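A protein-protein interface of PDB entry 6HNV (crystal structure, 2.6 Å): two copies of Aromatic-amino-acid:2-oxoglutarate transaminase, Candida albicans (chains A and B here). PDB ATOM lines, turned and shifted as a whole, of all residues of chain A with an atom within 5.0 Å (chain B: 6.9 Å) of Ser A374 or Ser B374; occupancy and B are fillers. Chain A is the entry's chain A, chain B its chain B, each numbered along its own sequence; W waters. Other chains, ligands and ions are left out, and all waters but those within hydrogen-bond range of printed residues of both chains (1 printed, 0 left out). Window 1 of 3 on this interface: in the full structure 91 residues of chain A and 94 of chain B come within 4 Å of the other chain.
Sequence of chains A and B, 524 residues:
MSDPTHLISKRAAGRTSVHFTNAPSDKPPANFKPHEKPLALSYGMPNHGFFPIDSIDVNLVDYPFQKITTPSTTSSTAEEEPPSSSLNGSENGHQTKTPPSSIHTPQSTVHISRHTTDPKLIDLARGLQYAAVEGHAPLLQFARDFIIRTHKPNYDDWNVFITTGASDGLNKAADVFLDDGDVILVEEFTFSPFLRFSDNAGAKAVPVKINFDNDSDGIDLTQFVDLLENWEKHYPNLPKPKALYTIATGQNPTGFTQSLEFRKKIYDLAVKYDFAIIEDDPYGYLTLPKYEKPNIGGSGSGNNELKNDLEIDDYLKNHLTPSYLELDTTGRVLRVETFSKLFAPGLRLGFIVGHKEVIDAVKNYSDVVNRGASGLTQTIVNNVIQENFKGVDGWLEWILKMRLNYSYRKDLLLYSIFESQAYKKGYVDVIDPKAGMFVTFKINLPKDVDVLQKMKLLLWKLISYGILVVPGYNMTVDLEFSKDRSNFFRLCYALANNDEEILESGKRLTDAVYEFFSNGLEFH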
ATOM      1  N   GLY A 346     -24.799 -23.483 -12.280  1.00  0.00           N
ATOM      2  CA  GLY A 346     -23.470 -23.223 -11.687  1.00  0.00           C
ATOM      3  C   GLY A 346     -22.565 -24.448 -11.706  1.00  0.00           C
ATOM      4  O   GLY A 346     -21.420 -24.341 -11.297  1.00  0.00           O
ATOM      5  N   LEU A 347     -23.028 -25.596 -12.196  1.00  0.00           N
ATOM      6  CA  LEU A 347     -22.113 -26.735 -12.483  1.00  0.00           C
ATOM      7  C   LEU A 347     -21.125 -26.356 -13.603  1.00  0.00           C
ATOM      8  O   LEU A 347     -19.904 -26.633 -13.434  1.00  0.00           O
ATOM      9  CB  LEU A 347     -22.900 -27.988 -12.870  1.00  0.00           C
ATOM     10  CG  LEU A 347     -23.947 -28.467 -11.877  1.00  0.00           C
ATOM     11  CD1 LEU A 347     -24.832 -29.472 -12.567  1.00  0.00           C
ATOM     12  CD2 LEU A 347     -23.316 -29.066 -10.641  1.00  0.00           C
ATOM     13  N   ARG A 348     -21.597 -25.720 -14.680  1.00  0.00           N
ATOM     14  CA  ARG A 348     -20.778 -25.530 -15.910  1.00  0.00           C
ATOM     15  C   ARG A 348     -20.383 -26.935 -16.396  1.00  0.00           C
ATOM     16  O   ARG A 348     -19.162 -27.198 -16.555  1.00  0.00           O
ATOM     17  CB  ARG A 348     -19.541 -24.636 -15.680  1.00  0.00           C
ATOM     18  CG  ARG A 348     -19.817 -23.269 -15.071  1.00  0.00           C
ATOM     19  CD  ARG A 348     -20.522 -22.277 -15.985  1.00  0.00           C
ATOM     20  NE  ARG A 348     -21.941 -22.561 -16.220  1.00  0.00           N
ATOM     21  CZ  ARG A 348     -22.590 -22.307 -17.356  1.00  0.00           C
ATOM     22  NH1 ARG A 348     -21.963 -21.765 -18.390  1.00  0.00           N
ATOM     23  NH2 ARG A 348     -23.864 -22.621 -17.464  1.00  0.00           N
ATOM     24  N   GLY A 372     -11.104 -28.889 -20.501  1.00  0.00           N
ATOM     25  CA  GLY A 372     -11.888 -29.864 -19.735  1.00  0.00           C
ATOM     26  C   GLY A 372     -12.742 -29.229 -18.653  1.00  0.00           C
ATOM     27  O   GLY A 372     -12.290 -28.263 -17.988  1.00  0.00           O
ATOM     28  N   ALA A 373     -13.949 -29.778 -18.488  1.00  0.00           N
ATOM     29  CA  ALA A 373     -14.885 -29.433 -17.399  1.00  0.00           C
ATOM     30  C   ALA A 373     -14.192 -29.672 -16.054  1.00  0.00           C
ATOM     31  O   ALA A 373     -13.247 -30.481 -15.995  1.00  0.00           O
ATOM     32  CB  ALA A 373     -16.156 -30.234 -17.550  1.00  0.00           C
ATOM     33  N   SER A 374     -14.609 -28.971 -15.007  1.00  0.00           N
ATOM     34  CA  SER A 374     -14.057 -29.193 -13.651  1.00  0.00           C
ATOM     35  C   SER A 374     -14.131 -30.699 -13.335  1.00  0.00           C
ATOM     36  O   SER A 374     -15.166 -31.317 -13.574  1.00  0.00           O
ATOM     37  CB  SER A 374     -14.759 -28.344 -12.623  1.00  0.00           C
ATOM     38  OG  SER A 374     -14.264 -28.643 -11.324  1.00  0.00           O
ATOM     39  N   GLY A 375     -13.041 -31.301 -12.888  1.00  0.00           N
ATOM     40  CA  GLY A 375     -13.051 -32.703 -12.449  1.00  0.00           C
ATOM     41  C   GLY A 375     -13.881 -32.852 -11.197  1.00  0.00           C
ATOM     42  O   GLY A 375     -14.634 -33.844 -11.108  1.00  0.00           O
ATOM     43  N   LEU A 376     -13.785 -31.895 -10.270  1.00  0.00           N
ATOM     44  CA  LEU A 376     -14.532 -31.976  -8.988  1.00  0.00           C
ATOM     45  C   LEU A 376     -16.031 -32.008  -9.301  1.00  0.00           C
ATOM     46  O   LEU A 376     -16.756 -32.793  -8.675  1.00  0.00           O
ATOM     47  CB  LEU A 376     -14.194 -30.800  -8.063  1.00  0.00           C
ATOM     48  CG  LEU A 376     -14.853 -30.880  -6.684  1.00  0.00           C
ATOM     49  CD1 LEU A 376     -14.529 -32.211  -6.020  1.00  0.00           C
ATOM     50  CD2 LEU A 376     -14.424 -29.714  -5.799  1.00  0.00           C
ATOM     51  N   THR A 377     -16.472 -31.162 -10.222  1.00  0.00           N
ATOM     52  CA  THR A 377     -17.884 -31.067 -10.661  1.00  0.00           C
ATOM     53  C   THR A 377     -18.299 -32.368 -11.370  1.00  0.00           C
ATOM     54  O   THR A 377     -19.411 -32.845 -11.103  1.00  0.00           O
ATOM     55  CB  THR A 377     -18.100 -29.828 -11.545  1.00  0.00           C
ATOM     56  OG1 THR A 377     -17.699 -28.648 -10.844  1.00  0.00           O
ATOM     57  CG2 THR A 377     -19.545 -29.651 -11.943  1.00  0.00           C
ATOM     58  N   GLN A 378     -17.461 -32.925 -12.251  1.00  0.00           N
ATOM     59  CA  GLN A 378     -17.786 -34.207 -12.936  1.00  0.00           C
ATOM     60  C   GLN A 378     -18.047 -35.236 -11.834  1.00  0.00           C
ATOM     61  O   GLN A 378     -19.018 -35.999 -11.963  1.00  0.00           O
ATOM     62  CB  GLN A 378     -16.690 -34.651 -13.915  1.00  0.00           C
ATOM     63  CG  GLN A 378     -16.716 -33.888 -15.239  1.00  0.00           C
ATOM     64  CD  GLN A 378     -15.526 -34.165 -16.129  1.00  0.00           C
ATOM     65  OE1 GLN A 378     -15.338 -35.260 -16.663  1.00  0.00           O
ATOM     66  NE2 GLN A 378     -14.724 -33.139 -16.327  1.00  0.00           N
ATOM     67  N   GLY B 127     -24.098 -20.443  -5.605  1.00  0.00           N
ATOM     68  CA  GLY B 127     -22.994 -21.274  -6.127  1.00  0.00           C
ATOM     69  C   GLY B 127     -23.407 -22.191  -7.271  1.00  0.00           C
ATOM     70  O   GLY B 127     -22.580 -22.393  -8.198  1.00  0.00           O
ATOM     71  N   HIS B 136     -17.349 -15.490  -8.818  1.00  0.00           N
ATOM     72  CA  HIS B 136     -18.078 -15.164  -7.564  1.00  0.00           C
ATOM     73  C   HIS B 136     -17.261 -14.155  -6.757  1.00  0.00           C
ATOM     74  O   HIS B 136     -16.021 -14.204  -6.801  1.00  0.00           O
ATOM     75  CB  HIS B 136     -18.388 -16.444  -6.786  1.00  0.00           C
ATOM     76  CG  HIS B 136     -19.519 -17.201  -7.377  1.00  0.00           C
ATOM     77  ND1 HIS B 136     -20.813 -17.007  -6.974  1.00  0.00           N
ATOM     78  CD2 HIS B 136     -19.561 -18.096  -8.387  1.00  0.00           C
ATOM     79  CE1 HIS B 136     -21.613 -17.765  -7.697  1.00  0.00           C
ATOM     80  NE2 HIS B 136     -20.869 -18.446  -8.577  1.00  0.00           N
ATOM     81  N   ILE B 162     -11.364 -14.853 -12.399  1.00  0.00           N
ATOM     82  CA  ILE B 162     -11.299 -16.317 -12.190  1.00  0.00           C
ATOM     83  C   ILE B 162     -11.257 -16.968 -13.566  1.00  0.00           C
ATOM     84  O   ILE B 162     -11.974 -16.489 -14.483  1.00  0.00           O
ATOM     85  CB  ILE B 162     -12.471 -16.821 -11.350  1.00  0.00           C
ATOM     86  CG1 ILE B 162     -12.486 -16.144  -9.980  1.00  0.00           C
ATOM     87  CG2 ILE B 162     -12.425 -18.337 -11.227  1.00  0.00           C
ATOM     88  CD1 ILE B 162     -11.278 -16.469  -9.099  1.00  0.00           C
ATOM     89  N   THR B 163     -10.423 -18.004 -13.675  1.00  0.00           N
ATOM     90  CA  THR B 163     -10.129 -18.782 -14.900  1.00  0.00           C
ATOM     91  C   THR B 163     -10.384 -20.255 -14.583  1.00  0.00           C
ATOM     92  O   THR B 163     -10.690 -20.535 -13.379  1.00  0.00           O
ATOM     93  CB  THR B 163      -8.665 -18.578 -15.309  1.00  0.00           C
ATOM     94  OG1 THR B 163      -7.845 -19.147 -14.289  1.00  0.00           O
ATOM     95  CG2 THR B 163      -8.293 -17.121 -15.491  1.00  0.00           C
ATOM     96  N   THR B 164     -10.243 -21.149 -15.579  1.00  0.00           N
ATOM     97  CA  THR B 164     -10.337 -22.618 -15.373  1.00  0.00           C
ATOM     98  C   THR B 164      -8.933 -23.226 -15.207  1.00  0.00           C
ATOM     99  O   THR B 164      -8.845 -24.458 -15.202  1.00  0.00           O
ATOM    100  CB  THR B 164     -11.247 -23.269 -16.421  1.00  0.00           C
ATOM    101  OG1 THR B 164     -10.879 -23.035 -17.786  1.00  0.00           O
ATOM    102  CG2 THR B 164     -12.663 -22.770 -16.247  1.00  0.00           C
ATOM    103  N   GLY B 346      -7.599 -31.168 -10.629  1.00  0.00           N
ATOM    104  CA  GLY B 346      -8.977 -31.454 -11.062  1.00  0.00           C
ATOM    105  C   GLY B 346      -9.959 -30.305 -10.838  1.00  0.00           C
ATOM    106  O   GLY B 346     -11.117 -30.437 -11.306  1.00  0.00           O
ATOM    107  N   LEU B 347      -9.578 -29.228 -10.138  1.00  0.00           N
ATOM    108  CA  LEU B 347     -10.502 -28.081  -9.913  1.00  0.00           C
ATOM    109  C   LEU B 347     -10.801 -27.412 -11.266  1.00  0.00           C
ATOM    110  O   LEU B 347     -11.964 -27.037 -11.527  1.00  0.00           O
ATOM    111  CB  LEU B 347      -9.890 -27.083  -8.926  1.00  0.00           C
ATOM    112  CG  LEU B 347      -9.719 -27.534  -7.471  1.00  0.00           C
ATOM    113  CD1 LEU B 347      -9.105 -26.395  -6.662  1.00  0.00           C
ATOM    114  CD2 LEU B 347     -11.028 -27.998  -6.818  1.00  0.00           C
ATOM    115  N   ARG B 348      -9.801 -27.344 -12.143  1.00  0.00           N
ATOM    116  CA  ARG B 348      -9.804 -26.418 -13.300  1.00  0.00           C
ATOM    117  C   ARG B 348     -10.137 -25.028 -12.748  1.00  0.00           C
ATOM    118  O   ARG B 348     -11.146 -24.467 -13.143  1.00  0.00           O
ATOM    119  CB  ARG B 348     -10.805 -26.859 -14.379  1.00  0.00           C
ATOM    120  CG  ARG B 348     -10.660 -28.289 -14.865  1.00  0.00           C
ATOM    121  CD  ARG B 348      -9.473 -28.500 -15.753  1.00  0.00           C
ATOM    122  NE  ARG B 348      -8.252 -28.562 -14.959  1.00  0.00           N
ATOM    123  CZ  ARG B 348      -7.045 -28.223 -15.399  1.00  0.00           C
ATOM    124  NH1 ARG B 348      -6.874 -27.793 -16.643  1.00  0.00           N
ATOM    125  NH2 ARG B 348      -6.003 -28.340 -14.588  1.00  0.00           N
ATOM    126  N   LEU B 349      -9.330 -24.515 -11.828  1.00  0.00           N
ATOM    127  CA  LEU B 349      -9.555 -23.170 -11.251  1.00  0.00           C
ATOM    128  C   LEU B 349      -8.234 -22.426 -11.121  1.00  0.00           C
ATOM    129  O   LEU B 349      -7.194 -23.029 -10.812  1.00  0.00           O
ATOM    130  CB  LEU B 349     -10.251 -23.264  -9.894  1.00  0.00           C
ATOM    131  CG  LEU B 349     -10.948 -21.970  -9.485  1.00  0.00           C
ATOM    132  CD1 LEU B 349     -12.110 -21.677 -10.432  1.00  0.00           C
ATOM    133  CD2 LEU B 349     -11.408 -22.037  -8.036  1.00  0.00           C
ATOM    134  N   ASN B 370     -15.242 -19.800 -23.120  1.00  0.00           N
ATOM    135  CA  ASN B 370     -15.197 -20.421 -21.760  1.00  0.00           C
ATOM    136  C   ASN B 370     -16.054 -19.570 -20.826  1.00  0.00           C
ATOM    137  O   ASN B 370     -15.492 -18.645 -20.234  1.00  0.00           O
ATOM    138  CB  ASN B 370     -13.780 -20.446 -21.198  1.00  0.00           C
ATOM    139  CG  ASN B 370     -13.579 -21.409 -20.057  1.00  0.00           C
ATOM    140  OD1 ASN B 370     -14.549 -21.897 -19.477  1.00  0.00           O
ATOM    141  ND2 ASN B 370     -12.317 -21.706 -19.765  1.00  0.00           N
ATOM    142  N   GLY B 372     -17.414 -19.127 -17.850  1.00  0.00           N
ATOM    143  CA  GLY B 372     -17.409 -19.298 -16.389  1.00  0.00           C
ATOM    144  C   GLY B 372     -16.643 -20.520 -15.916  1.00  0.00           C
ATOM    145  O   GLY B 372     -16.800 -21.601 -16.475  1.00  0.00           O
ATOM    146  N   ALA B 373     -15.828 -20.354 -14.881  1.00  0.00           N
ATOM    147  CA  ALA B 373     -15.312 -21.484 -14.076  1.00  0.00           C
ATOM    148  C   ALA B 373     -16.492 -22.125 -13.352  1.00  0.00           C
ATOM    149  O   ALA B 373     -17.449 -21.433 -13.035  1.00  0.00           O
ATOM    150  CB  ALA B 373     -14.232 -21.009 -13.118  1.00  0.00           C
ATOM    151  N   SER B 374     -16.401 -23.413 -13.062  1.00  0.00           N
ATOM    152  CA  SER B 374     -17.477 -24.157 -12.362  1.00  0.00           C
ATOM    153  C   SER B 374     -17.804 -23.468 -11.030  1.00  0.00           C
ATOM    154  O   SER B 374     -16.935 -23.396 -10.159  1.00  0.00           O
ATOM    155  CB  SER B 374     -17.078 -25.585 -12.165  1.00  0.00           C
ATOM    156  OG  SER B 374     -18.120 -26.312 -11.532  1.00  0.00           O
ATOM    157  N   GLY B 375     -19.017 -22.954 -10.900  1.00  0.00           N
ATOM    158  CA  GLY B 375     -19.538 -22.280  -9.696  1.00  0.00           C
ATOM    159  C   GLY B 375     -19.520 -23.190  -8.495  1.00  0.00           C
ATOM    160  O   GLY B 375     -19.246 -22.658  -7.408  1.00  0.00           O
ATOM    161  N   LEU B 376     -19.779 -24.498  -8.665  1.00  0.00           N
ATOM    162  CA  LEU B 376     -19.751 -25.499  -7.555  1.00  0.00           C
ATOM    163  C   LEU B 376     -18.315 -25.615  -7.057  1.00  0.00           C
ATOM    164  O   LEU B 376     -18.112 -25.933  -5.882  1.00  0.00           O
ATOM    165  CB  LEU B 376     -20.267 -26.876  -8.007  1.00  0.00           C
ATOM    166  CG  LEU B 376     -20.184 -28.002  -6.965  1.00  0.00           C
ATOM    167  CD1 LEU B 376     -20.741 -27.554  -5.628  1.00  0.00           C
ATOM    168  CD2 LEU B 376     -20.937 -29.250  -7.418  1.00  0.00           C
ATOM    169  N   THR B 377     -17.350 -25.442  -7.952  1.00  0.00           N
ATOM    170  CA  THR B 377     -15.915 -25.620  -7.633  1.00  0.00           C
ATOM    171  C   THR B 377     -15.433 -24.360  -6.917  1.00  0.00           C
ATOM    172  O   THR B 377     -14.725 -24.502  -5.893  1.00  0.00           O
ATOM    173  CB  THR B 377     -15.118 -25.955  -8.895  1.00  0.00           C
ATOM    174  OG1 THR B 377     -15.708 -27.142  -9.420  1.00  0.00           O
ATOM    175  CG2 THR B 377     -13.652 -26.190  -8.621  1.00  0.00           C
ATOM    176  N   GLN B 378     -15.823 -23.192  -7.449  1.00  0.00           N
ATOM    177  CA  GLN B 378     -15.554 -21.853  -6.865  1.00  0.00           C
ATOM    178  C   GLN B 378     -16.138 -21.853  -5.443  1.00  0.00           C
ATOM    179  O   GLN B 378     -15.504 -21.332  -4.527  1.00  0.00           O
ATOM    180  CB  GLN B 378     -16.129 -20.754  -7.767  1.00  0.00           C
ATOM    181  CG  GLN B 378     -15.424 -20.543  -9.116  1.00  0.00           C
ATOM    182  CD  GLN B 378     -15.993 -19.330  -9.832  1.00  0.00           C
ATOM    183  OE1 GLN B 378     -16.047 -18.232  -9.272  1.00  0.00           O
ATOM    184  NE2 GLN B 378     -16.470 -19.507 -11.060  1.00  0.00           N
ATOM    185  N   THR B 379     -17.290 -22.485  -5.256  1.00  0.00           N
ATOM    186  CA  THR B 379     -17.976 -22.614  -3.938  1.00  0.00           C
ATOM    187  C   THR B 379     -17.115 -23.468  -2.987  1.00  0.00           C
ATOM    188  O   THR B 379     -16.704 -22.938  -1.920  1.00  0.00           O
ATOM    189  CB  THR B 379     -19.406 -23.150  -4.136  1.00  0.00           C
ATOM    190  OG1 THR B 379     -20.050 -22.368  -5.142  1.00  0.00           O
ATOM    191  CG2 THR B 379     -20.247 -23.107  -2.879  1.00  0.00           C
HETATM  192  O   HOH W   1     -11.116 -25.568 -18.768  1.00  0.00           O
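Printed residues of chain B within 4 Å of Gly A346: Gly B127, Ser B374, Gly B375 and Leu B376. Ser A374 touches just these residues of chain B: Gly B346 (3.6 Å), Leu B347 (2.8 Å), Arg B348 (3.7 Å), Ser B374 (3.6 Å) and Thr B377 (2.8 Å). Thr B163 touches none of the printed residues of chain A. Printed residues of chain A within 4 Å of Ala B373: Arg A348 (3.6 Å). Gln B378 touches none of the printed residues of chain A. The nearest printed residue of chain A that does not touch Ser B374 is Ala A373 (6.3 Å).
NE2 of Gln A378 lies within hydrogen-bond range of O of Ser A374, at 3.3 Å. The backbone carbonyl oxygen of Gly B375 sits at hydrogen-bond distance from the side-chain hydroxyl of Thr B379 (2.4 Å). OG of Ser A374 sits close to N of Leu A376 (3.5 Å). OG1 of Thr A377 sits close to OG of Ser A374 (3.5 Å). The side-chain hydroxyl of Thr B377 sits at hydrogen-bond distance from the side-chain hydroxyl of Ser B374 (3.3 Å). O of Ala A373 sits at hydrogen-bond distance from NE2 of Gln A378 (3.1 Å).
Of the 10 printed residues of chain A, 9 touch a printed residue of chain B. Printed residues of chain A that touch a printed residue of chain B: Gly A346, Leu A347, Arg A348, Gly A372, Ala A373, Ser A374, Gly A375, Leu A376 and Thr A377. Hydrophobic or aromatic side chains of chain A within 4 Å of the printed part of chain B: Leu A376. Along chain A the printed residues that touch a printed residue of chain B span positions 346 to 377. Of the 18 printed residues of chain B, 10 touch a printed residue of chain A. Hydrophobic or aromatic side chains of chain B that line the printed part of chain A: Leu B347. Among the printed residues, no Asp or Glu carboxylate lies within 4 Å of a Lys or Arg side-chain nitrogen of the other chain.
Among the printed residues, pairs that only touch across the chains: Gly A346 with Gly B127, Gly A346 with Ser B374, Arg A348 with Gly B372, Arg A348 with Ala B373, Arg A348 with Ser B374, Gly A372 with Arg B348, Ala A373 with Arg B348, Ser A374 with Gly B346, Ser A374 with Arg B348, Ser A374 with Ser B374 and Leu A376 with Leu B347.
The backbone NH (N) of Leu B376 is in hydrogen-bond range of the backbone carbonyl oxygen (O) of Gly A346, at 3.1 Å. OG of Ser A374 lies within hydrogen-bond range of O of Leu B347, at 2.8 Å. The backbone NH (N) of Leu A376 sits at hydrogen-bond distance from the backbone carbonyl oxygen (O) of Gly B346 (3.2 Å). OG1 of Thr B377 sits at hydrogen-bond distance from OG1 of Thr A377. The backbone carbonyl oxygen (O) of Gly B346 lies within hydrogen-bond range of the backbone NH (N) of Gly A375 (2.6 Å). O of Gly A346 is in hydrogen-bond range of N of Gly B375 (2.8 Å). The side-chain hydroxyl (OG1) of Thr B377 is in hydrogen-bond range of the side-chain hydroxyl (OG) of Ser A374 (2.8 Å). OG1 of Thr A377 is in hydrogen-bond range of OG of Ser B374 (2.5 Å). The side-chain hydroxyl of Ser B374 lies within hydrogen-bond range of the backbone carbonyl oxygen of Leu A347 (2.6 Å).
Arg A348 touches Ser B374, and with the chains exchanged Ser A374 touches Arg B348. Ser A374 touches its own counterpart, Ser B374. Ser A374 touches Thr B377, and with the chains exchanged Thr A377 touches Ser B374. Thr A377 touches its own counterpart, Thr B377.
Water W1 lies within hydrogen-bond range of the side-chain hydroxyl (OG1) of Thr B164 and the backbone carbonyl oxygen (O) of Gly A372.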
